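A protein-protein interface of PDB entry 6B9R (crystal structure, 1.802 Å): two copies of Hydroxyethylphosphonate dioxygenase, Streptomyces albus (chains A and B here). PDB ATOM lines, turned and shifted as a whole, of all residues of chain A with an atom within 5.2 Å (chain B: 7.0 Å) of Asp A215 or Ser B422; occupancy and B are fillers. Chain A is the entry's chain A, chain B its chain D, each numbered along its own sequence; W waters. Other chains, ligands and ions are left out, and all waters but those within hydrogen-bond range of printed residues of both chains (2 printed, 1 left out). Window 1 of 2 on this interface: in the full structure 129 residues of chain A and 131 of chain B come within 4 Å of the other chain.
The side-chain amide oxygen (OE1) of Gln A217 sits at hydrogen-bond distance from the guanidinium group (NH1) of Arg A218.
The guanidinium group (NH1) of Arg B73 lies within salt-bridge range of the side-chain carboxylate (OD1) of Asp B215 (2.6 Å).
The backbone carbonyl oxygen of Gly B214 lies close to the guanidinium group of Arg B218 (3.5 Å).
The backbone carbonyl oxygen (O) of Gly A214 lies within hydrogen-bond range of the guanidinium group (NH1) of Arg A218, 3.3 Å away.
The backbone NH of Val B427 is in hydrogen-bond range of the side-chain hydroxyl of Thr B424.
O of Gly B210 is in hydrogen-bond range of OG1 of Thr B213 (3.4 Å).
Water W1 lies within hydrogen-bond range of OD2 of Asp A215 and O of Thr B213.
Water W2 bridges the backbone carbonyl oxygen of Arg A218 (3.0 Å) and the backbone NH of Ile B78 (3.1 Å).
The side-chain carboxylate (OE1) of Glu A219 is in hydrogen-bond range of a ring nitrogen (NE2) of His B364, at 3.0 Å.
The side-chain carboxylate of Asp B215 lies within salt-bridge range of the guanidinium group of Arg A73 (3.5 Å).
NH2 of Arg B73 is in salt-bridge range of OD1 of Asp A215 (3.1 Å).
The guanidinium group of Arg B73 sits at hydrogen-bond distance from the backbone carbonyl oxygen of Arg A73.
NE2 of Gln A217 sits at hydrogen-bond distance from O of Tyr B442 (3.0 Å).
The side-chain carboxylate of Glu A219 sits at hydrogen-bond distance from the side-chain hydroxyl of Ser B422.
The backbone NH (N) of Asp A215 lies within hydrogen-bond range of the side-chain carboxylate (OD2) of Asp B215 (2.7 Å).
Of the printed residues of chain B, Asp A215 touches Arg B73, Thr B213, Gly B214, Asp B215 and Ser B422.
Printed residues of chain A within 4 Å of His B364: Glu A219.
Of the printed residues of chain A, Arg B218 touches Arg A73.
The nearest printed residue of chain B that does not touch Asp A215 is Ala B216 (5.1 Å).
The nearest printed residue of chain A that does not touch Thr B213 is Arg A73 (8.0 Å).
Asp B215 touches Gly A214.
Thr B213 touches Asp A215 (O to OD2, 3.996 Å).
CA of Gly B214 touches OD2 of Asp A215, 3.5 Å away.
OG of Ser B422 touches CB of Asp A215, 3.4 Å away.
Ser B422 touches Ala A216 (O to CB, 3.6 Å).
Ala A216 touches Tyr B442 (C to OH, 3.7 Å).
CG1 of Ile B78 touches O of Arg A218 (3.4 Å).
Glu A219 touches Ile B78 (CA to CD1, 3.8 Å).
Gly B421 touches Glu A219.
Leu A220 touches Tyr B442 (CD1 to OH, 3.8 Å).
Arg A73 touches Asp B215, and with the chains exchanged Asp A215 touches Arg B73.
Arg A73 touches Arg B218, but with the chains exchanged Arg A218 does not touch Arg B73 (4.4 Å).
Gly A214 touches Asp B215, and with the chains exchanged Asp A215 touches Gly B214.
Asp B215 touches its own counterpart, Asp A215.
Of the 20 pairs that touch across the chains among the printed residues, 6 have their exchanged pair printed and touching as well.
Hydrophobic or aromatic side chains of chain B that line the printed part of chain A: Ile B78, His B364, Val B427 and Tyr B442.
Hydrophobic or aromatic side chains of chain A that line the printed part of chain B: Ala A216 and Leu A220.
Among the printed residues, 20 pairs touch across the chains.
Among the printed residues, Asp or Glu carboxylates within 4 Å of a Lys or Arg side-chain nitrogen of the other chain: Arg A73 with Asp B215 (3.5 Å) and Asp A215 with Arg B73 (3.1 Å).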
ATOM      1  N   ARG A  73      22.473 -23.704   1.781  1.00  0.00           N
ATOM      2  CA  ARG A  73      22.931 -24.311   0.535  1.00  0.00           C
ATOM      3  C   ARG A  73      23.908 -23.414  -0.218  1.00  0.00           C
ATOM      4  O   ARG A  73      24.794 -23.915  -0.923  1.00  0.00           O
ATOM      5  CB  ARG A  73      21.725 -24.615  -0.363  1.00  0.00           C
ATOM      6  CG  ARG A  73      21.545 -26.036  -0.754  1.00  0.00           C
ATOM      7  CD  ARG A  73      20.321 -26.219  -1.678  1.00  0.00           C
ATOM      8  NE  ARG A  73      20.565 -27.256  -2.686  1.00  0.00           N
ATOM      9  CZ  ARG A  73      20.725 -27.009  -3.983  1.00  0.00           C
ATOM     10  NH1 ARG A  73      20.943 -28.001  -4.832  1.00  0.00           N
ATOM     11  NH2 ARG A  73      20.671 -25.765  -4.426  1.00  0.00           N
ATOM     12  N   THR A 213      16.689 -31.744 -11.212  1.00  0.00           N
ATOM     13  CA  THR A 213      17.152 -31.916  -9.842  1.00  0.00           C
ATOM     14  C   THR A 213      18.115 -30.787  -9.463  1.00  0.00           C
ATOM     15  O   THR A 213      18.605 -30.039 -10.306  1.00  0.00           O
ATOM     16  CB  THR A 213      17.816 -33.285  -9.680  1.00  0.00           C
ATOM     17  OG1 THR A 213      18.808 -33.461 -10.701  1.00  0.00           O
ATOM     18  CG2 THR A 213      16.771 -34.389  -9.815  1.00  0.00           C
ATOM     19  N   GLY A 214      18.385 -30.658  -8.175  1.00  0.00           N
ATOM     20  CA  GLY A 214      19.222 -29.550  -7.763  1.00  0.00           C
ATOM     21  C   GLY A 214      18.467 -28.237  -7.673  1.00  0.00           C
ATOM     22  O   GLY A 214      17.321 -28.226  -7.212  1.00  0.00           O
ATOM     23  N   ASP A 215      19.097 -27.133  -8.114  1.00  0.00           N
ATOM     24  CA  ASP A 215      18.588 -25.797  -7.806  1.00  0.00           C
ATOM     25  C   ASP A 215      17.138 -25.627  -8.247  1.00  0.00           C
ATOM     26  O   ASP A 215      16.338 -24.990  -7.548  1.00  0.00           O
ATOM     27  CB  ASP A 215      19.447 -24.722  -8.480  1.00  0.00           C
ATOM     28  CG  ASP A 215      20.855 -24.612  -7.889  1.00  0.00           C
ATOM     29  OD1 ASP A 215      21.100 -25.060  -6.751  1.00  0.00           O
ATOM     30  OD2 ASP A 215      21.728 -24.072  -8.590  1.00  0.00           O
ATOM     31  N   ALA A 216      16.787 -26.166  -9.418  1.00  0.00           N
ATOM     32  CA  ALA A 216      15.434 -25.974  -9.940  1.00  0.00           C
ATOM     33  C   ALA A 216      14.394 -26.580  -9.010  1.00  0.00           C
ATOM     34  O   ALA A 216      13.351 -25.966  -8.750  1.00  0.00           O
ATOM     35  CB  ALA A 216      15.318 -26.570 -11.345  1.00  0.00           C
ATOM     36  N   GLN A 217      14.671 -27.767  -8.472  1.00  0.00           N
ATOM     37  CA  GLN A 217      13.725 -28.403  -7.557  1.00  0.00           C
ATOM     38  C   GLN A 217      13.541 -27.572  -6.294  1.00  0.00           C
ATOM     39  O   GLN A 217      12.414 -27.382  -5.826  1.00  0.00           O
ATOM     40  CB  GLN A 217      14.213 -29.808  -7.196  1.00  0.00           C
ATOM     41  CG  GLN A 217      13.196 -30.704  -6.486  1.00  0.00           C
ATOM     42  CD  GLN A 217      13.003 -30.374  -5.018  1.00  0.00           C
ATOM     43  OE1 GLN A 217      13.867 -29.775  -4.383  1.00  0.00           O
ATOM     44  NE2 GLN A 217      11.850 -30.758  -4.472  1.00  0.00           N
ATOM     45  N   ARG A 218      14.644 -27.084  -5.722  1.00  0.00           N
ATOM     46  CA  ARG A 218      14.563 -26.316  -4.480  1.00  0.00           C
ATOM     47  C   ARG A 218      13.732 -25.061  -4.666  1.00  0.00           C
ATOM     48  O   ARG A 218      12.898 -24.724  -3.817  1.00  0.00           O
ATOM     49  CB  ARG A 218      15.968 -25.933  -4.006  1.00  0.00           C
ATOM     50  CG  ARG A 218      16.934 -27.090  -3.898  1.00  0.00           C
ATOM     51  CD  ARG A 218      16.527 -28.069  -2.823  1.00  0.00           C
ATOM     52  NE  ARG A 218      17.491 -29.163  -2.710  1.00  0.00           N
ATOM     53  CZ  ARG A 218      17.617 -30.145  -3.592  1.00  0.00           C
ATOM     54  NH1 ARG A 218      16.834 -30.187  -4.653  1.00  0.00           N
ATOM     55  NH2 ARG A 218      18.526 -31.094  -3.406  1.00  0.00           N
ATOM     56  N   GLU A 219      13.956 -24.354  -5.771  1.00  0.00           N
ATOM     57  CA  GLU A 219      13.231 -23.120  -6.042  1.00  0.00           C
ATOM     58  C   GLU A 219      11.760 -23.405  -6.290  1.00  0.00           C
ATOM     59  O   GLU A 219      10.875 -22.830  -5.647  1.00  0.00           O
ATOM     60  CB  GLU A 219      13.859 -22.437  -7.257  1.00  0.00           C
ATOM     61  CG  GLU A 219      13.837 -20.940  -7.250  1.00  0.00           C
ATOM     62  CD  GLU A 219      14.538 -20.362  -8.474  1.00  0.00           C
ATOM     63  OE1 GLU A 219      13.838 -20.030  -9.452  1.00  0.00           O
ATOM     64  OE2 GLU A 219      15.782 -20.249  -8.447  1.00  0.00           O
ATOM     65  N   LEU A 220      11.479 -24.310  -7.221  1.00  0.00           N
ATOM     66  CA  LEU A 220      10.089 -24.603  -7.539  1.00  0.00           C
ATOM     67  C   LEU A 220       9.336 -25.135  -6.330  1.00  0.00           C
ATOM     68  O   LEU A 220       8.139 -24.858  -6.172  1.00  0.00           O
ATOM     69  CB  LEU A 220      10.036 -25.597  -8.688  1.00  0.00           C
ATOM     70  CG  LEU A 220      10.517 -25.013 -10.014  1.00  0.00           C
ATOM     71  CD1 LEU A 220      10.630 -26.122 -11.050  1.00  0.00           C
ATOM     72  CD2 LEU A 220       9.569 -23.933 -10.489  1.00  0.00           C
ATOM     73  N   ARG B  73      24.801 -30.510   0.698  1.00  0.00           N
ATOM     74  CA  ARG B  73      24.009 -29.555  -0.060  1.00  0.00           C
ATOM     75  C   ARG B  73      22.764 -30.202  -0.662  1.00  0.00           C
ATOM     76  O   ARG B  73      21.695 -29.577  -0.729  1.00  0.00           O
ATOM     77  CB  ARG B  73      24.904 -28.953  -1.148  1.00  0.00           C
ATOM     78  CG  ARG B  73      24.519 -27.601  -1.638  1.00  0.00           C
ATOM     79  CD  ARG B  73      25.459 -27.121  -2.748  1.00  0.00           C
ATOM     80  NE  ARG B  73      24.876 -25.950  -3.394  1.00  0.00           N
ATOM     81  CZ  ARG B  73      24.226 -25.988  -4.549  1.00  0.00           C
ATOM     82  NH1 ARG B  73      24.094 -27.138  -5.190  1.00  0.00           N
ATOM     83  NH2 ARG B  73      23.707 -24.884  -5.065  1.00  0.00           N
ATOM     84  N   ILE B  78      15.741 -24.849   0.234  1.00  0.00           N
ATOM     85  CA  ILE B  78      15.939 -23.421   0.395  1.00  0.00           C
ATOM     86  C   ILE B  78      14.790 -22.870   1.230  1.00  0.00           C
ATOM     87  O   ILE B  78      13.779 -23.531   1.451  1.00  0.00           O
ATOM     88  CB  ILE B  78      16.082 -22.681  -0.959  1.00  0.00           C
ATOM     89  CG1 ILE B  78      14.789 -22.712  -1.756  1.00  0.00           C
ATOM     90  CG2 ILE B  78      17.244 -23.252  -1.771  1.00  0.00           C
ATOM     91  CD1 ILE B  78      14.769 -21.658  -2.861  1.00  0.00           C
ATOM     92  N   GLN B 119      14.771 -16.936  -2.346  1.00  0.00           N
ATOM     93  CA  GLN B 119      14.268 -17.695  -3.487  1.00  0.00           C
ATOM     94  C   GLN B 119      14.792 -17.196  -4.838  1.00  0.00           C
ATOM     95  O   GLN B 119      14.465 -17.796  -5.868  1.00  0.00           O
ATOM     96  CB  GLN B 119      12.732 -17.665  -3.471  1.00  0.00           C
ATOM     97  CG  GLN B 119      12.154 -18.308  -2.204  1.00  0.00           C
ATOM     98  CD  GLN B 119      10.737 -17.867  -1.906  1.00  0.00           C
ATOM     99  OE1 GLN B 119      10.514 -16.935  -1.126  1.00  0.00           O
ATOM    100  NE2 GLN B 119       9.765 -18.546  -2.507  1.00  0.00           N
ATOM    101  N   GLY B 210      22.762 -15.897 -12.651  1.00  0.00           N
ATOM    102  CA  GLY B 210      21.970 -16.645 -13.590  1.00  0.00           C
ATOM    103  C   GLY B 210      22.450 -18.065 -13.618  1.00  0.00           C
ATOM    104  O   GLY B 210      22.514 -18.741 -12.582  1.00  0.00           O
ATOM    105  N   GLU B 211      22.833 -18.505 -14.814  1.00  0.00           N
ATOM    106  CA  GLU B 211      23.290 -19.872 -14.990  1.00  0.00           C
ATOM    107  C   GLU B 211      24.515 -20.169 -14.118  1.00  0.00           C
ATOM    108  O   GLU B 211      24.671 -21.285 -13.606  1.00  0.00           O
ATOM    109  CB  GLU B 211      23.576 -20.096 -16.484  1.00  0.00           C
ATOM    110  N   THR B 213      25.649 -19.162 -11.086  1.00  0.00           N
ATOM    111  CA  THR B 213      25.638 -19.332  -9.644  1.00  0.00           C
ATOM    112  C   THR B 213      24.892 -20.605  -9.261  1.00  0.00           C
ATOM    113  O   THR B 213      23.936 -21.018  -9.919  1.00  0.00           O
ATOM    114  CB  THR B 213      25.022 -18.105  -8.958  1.00  0.00           C
ATOM    115  OG1 THR B 213      23.737 -17.814  -9.523  1.00  0.00           O
ATOM    116  CG2 THR B 213      25.917 -16.885  -9.144  1.00  0.00           C
ATOM    117  N   GLY B 214      25.339 -21.236  -8.192  1.00  0.00           N
ATOM    118  CA  GLY B 214      24.683 -22.427  -7.681  1.00  0.00           C
ATOM    119  C   GLY B 214      25.334 -23.705  -8.208  1.00  0.00           C
ATOM    120  O   GLY B 214      26.559 -23.838  -8.191  1.00  0.00           O
ATOM    121  N   ASP B 215      24.501 -24.650  -8.652  1.00  0.00           N
ATOM    122  CA  ASP B 215      24.985 -25.978  -9.039  1.00  0.00           C
ATOM    123  C   ASP B 215      26.188 -25.907  -9.975  1.00  0.00           C
ATOM    124  O   ASP B 215      27.165 -26.643  -9.802  1.00  0.00           O
ATOM    125  CB  ASP B 215      23.863 -26.783  -9.712  1.00  0.00           C
ATOM    126  CG  ASP B 215      22.784 -27.222  -8.734  1.00  0.00           C
ATOM    127  OD1 ASP B 215      23.100 -27.414  -7.541  1.00  0.00           O
ATOM    128  OD2 ASP B 215      21.615 -27.373  -9.155  1.00  0.00           O
ATOM    129  N   ALA B 216      26.108 -25.080 -11.022  1.00  0.00           N
ATOM    130  CA  ALA B 216      27.176 -25.091 -12.017  1.00  0.00           C
ATOM    131  C   ALA B 216      28.502 -24.676 -11.389  1.00  0.00           C
ATOM    132  O   ALA B 216      29.534 -25.316 -11.625  1.00  0.00           O
ATOM    133  CB  ALA B 216      26.806 -24.186 -13.200  1.00  0.00           C
ATOM    134  N   ARG B 218      29.343 -25.078  -8.282  1.00  0.00           N
ATOM    135  CA  ARG B 218      29.782 -26.158  -7.399  1.00  0.00           C
ATOM    136  C   ARG B 218      30.503 -27.250  -8.181  1.00  0.00           C
ATOM    137  O   ARG B 218      31.552 -27.740  -7.754  1.00  0.00           O
ATOM    138  CB  ARG B 218      28.590 -26.754  -6.649  1.00  0.00           C
ATOM    139  CG  ARG B 218      27.822 -25.750  -5.787  1.00  0.00           C
ATOM    140  CD  ARG B 218      28.707 -25.094  -4.741  1.00  0.00           C
ATOM    141  NE  ARG B 218      27.915 -24.232  -3.862  1.00  0.00           N
ATOM    142  CZ  ARG B 218      27.547 -22.994  -4.168  1.00  0.00           C
ATOM    143  NH1 ARG B 218      27.924 -22.460  -5.322  1.00  0.00           N
ATOM    144  NH2 ARG B 218      26.812 -22.281  -3.319  1.00  0.00           N
ATOM    145  N   HIS B 364      11.412 -14.247 -12.178  1.00  0.00           N
ATOM    146  CA  HIS B 364      11.302 -13.445 -10.962  1.00  0.00           C
ATOM    147  C   HIS B 364      11.143 -11.977 -11.344  1.00  0.00           C
ATOM    148  O   HIS B 364      11.553 -11.549 -12.426  1.00  0.00           O
ATOM    149  CB  HIS B 364      12.551 -13.577 -10.084  1.00  0.00           C
ATOM    150  CG  HIS B 364      12.849 -14.969  -9.625  1.00  0.00           C
ATOM    151  ND1 HIS B 364      12.463 -15.442  -8.391  1.00  0.00           N
ATOM    152  CD2 HIS B 364      13.504 -15.990 -10.230  1.00  0.00           C
ATOM    153  CE1 HIS B 364      12.863 -16.695  -8.255  1.00  0.00           C
ATOM    154  NE2 HIS B 364      13.493 -17.053  -9.358  1.00  0.00           N
ATOM    155  N   GLY B 420      15.493 -14.589 -15.249  1.00  0.00           N
ATOM    156  CA  GLY B 420      15.235 -16.013 -15.202  1.00  0.00           C
ATOM    157  C   GLY B 420      15.745 -16.599 -13.898  1.00  0.00           C
ATOM    158  O   GLY B 420      16.777 -16.180 -13.366  1.00  0.00           O
ATOM    159  N   GLY B 421      15.001 -17.564 -13.367  1.00  0.00           N
ATOM    160  CA  GLY B 421      15.433 -18.332 -12.219  1.00  0.00           C
ATOM    161  C   GLY B 421      16.033 -19.664 -12.624  1.00  0.00           C
ATOM    162  O   GLY B 421      16.417 -19.883 -13.778  1.00  0.00           O
ATOM    163  N   SER B 422      16.101 -20.578 -11.652  1.00  0.00           N
ATOM    164  CA  SER B 422      16.630 -21.908 -11.915  1.00  0.00           C
ATOM    165  C   SER B 422      15.709 -22.739 -12.801  1.00  0.00           C
ATOM    166  O   SER B 422      16.166 -23.728 -13.381  1.00  0.00           O
ATOM    167  CB  SER B 422      16.879 -22.642 -10.595  1.00  0.00           C
ATOM    168  OG  SER B 422      17.959 -22.062  -9.884  1.00  0.00           O
ATOM    169  N   ALA B 423      14.427 -22.371 -12.912  1.00  0.00           N
ATOM    170  CA  ALA B 423      13.520 -23.026 -13.859  1.00  0.00           C
ATOM    171  C   ALA B 423      13.798 -22.448 -15.245  1.00  0.00           C
ATOM    172  O   ALA B 423      13.157 -21.503 -15.713  1.00  0.00           O
ATOM    173  CB  ALA B 423      12.065 -22.842 -13.440  1.00  0.00           C
ATOM    174  N   THR B 424      14.814 -23.021 -15.888  1.00  0.00           N
ATOM    175  CA  THR B 424      15.260 -22.652 -17.217  1.00  0.00           C
ATOM    176  C   THR B 424      14.275 -23.189 -18.247  1.00  0.00           C
ATOM    177  O   THR B 424      13.402 -23.993 -17.917  1.00  0.00           O
ATOM    178  CB  THR B 424      16.639 -23.251 -17.475  1.00  0.00           C
ATOM    179  OG1 THR B 424      16.523 -24.671 -17.356  1.00  0.00           O
ATOM    180  CG2 THR B 424      17.646 -22.743 -16.445  1.00  0.00           C
ATOM    181  N   PRO B 425      14.390 -22.775 -19.513  1.00  0.00           N
ATOM    182  CA  PRO B 425      13.541 -23.399 -20.534  1.00  0.00           C
ATOM    183  C   PRO B 425      13.625 -24.917 -20.507  1.00  0.00           C
ATOM    184  O   PRO B 425      12.590 -25.584 -20.625  1.00  0.00           O
ATOM    185  CB  PRO B 425      14.077 -22.807 -21.847  1.00  0.00           C
ATOM    186  CG  PRO B 425      14.642 -21.472 -21.434  1.00  0.00           C
ATOM    187  CD  PRO B 425      15.255 -21.720 -20.086  1.00  0.00           C
ATOM    188  N   VAL B 427      14.228 -26.843 -17.954  1.00  0.00           N
ATOM    189  CA  VAL B 427      13.413 -27.295 -16.828  1.00  0.00           C
ATOM    190  C   VAL B 427      11.936 -27.259 -17.205  1.00  0.00           C
ATOM    191  O   VAL B 427      11.175 -28.185 -16.903  1.00  0.00           O
ATOM    192  CB  VAL B 427      13.685 -26.436 -15.577  1.00  0.00           C
ATOM    193  CG1 VAL B 427      12.636 -26.715 -14.517  1.00  0.00           C
ATOM    194  CG2 VAL B 427      15.093 -26.700 -15.020  1.00  0.00           C
ATOM    195  N   ARG B 428      11.508 -26.178 -17.860  1.00  0.00           N
ATOM    196  CA  ARG B 428      10.093 -26.021 -18.187  1.00  0.00           C
ATOM    197  C   ARG B 428       9.645 -27.039 -19.232  1.00  0.00           C
ATOM    198  O   ARG B 428       8.521 -27.543 -19.160  1.00  0.00           O
ATOM    199  CB  ARG B 428       9.834 -24.589 -18.647  1.00  0.00           C
ATOM    200  CG  ARG B 428      10.194 -23.560 -17.557  1.00  0.00           C
ATOM    201  CD  ARG B 428      10.092 -22.145 -18.108  1.00  0.00           C
ATOM    202  NE  ARG B 428       8.712 -21.823 -18.457  1.00  0.00           N
ATOM    203  CZ  ARG B 428       8.350 -20.890 -19.333  1.00  0.00           C
ATOM    204  NH1 ARG B 428       7.063 -20.658 -19.562  1.00  0.00           N
ATOM    205  NH2 ARG B 428       9.269 -20.208 -19.991  1.00  0.00           N
ATOM    206  N   TYR B 442       7.304 -34.317  -7.351  1.00  0.00           N
ATOM    207  CA  TYR B 442       8.542 -33.633  -7.694  1.00  0.00           C
ATOM    208  C   TYR B 442       8.869 -32.562  -6.660  1.00  0.00           C
ATOM    209  O   TYR B 442      10.024 -32.409  -6.244  1.00  0.00           O
ATOM    210  CB  TYR B 442       8.422 -33.036  -9.096  1.00  0.00           C
ATOM    211  CG  TYR B 442       9.518 -32.063  -9.454  1.00  0.00           C
ATOM    212  CD1 TYR B 442      10.850 -32.463  -9.469  1.00  0.00           C
ATOM    213  CD2 TYR B 442       9.230 -30.751  -9.780  1.00  0.00           C
ATOM    214  CE1 TYR B 442      11.864 -31.575  -9.797  1.00  0.00           C
ATOM    215  CE2 TYR B 442      10.242 -29.863 -10.119  1.00  0.00           C
ATOM    216  CZ  TYR B 442      11.551 -30.285 -10.123  1.00  0.00           C
ATOM    217  OH  TYR B 442      12.553 -29.402 -10.455  1.00  0.00           O
HETATM  218  O   HOH W   1      21.421 -23.053 -10.753  1.00  0.00           O
HETATM  219  O   HOH W   2      13.272 -26.029  -1.153  1.00  0.00           O
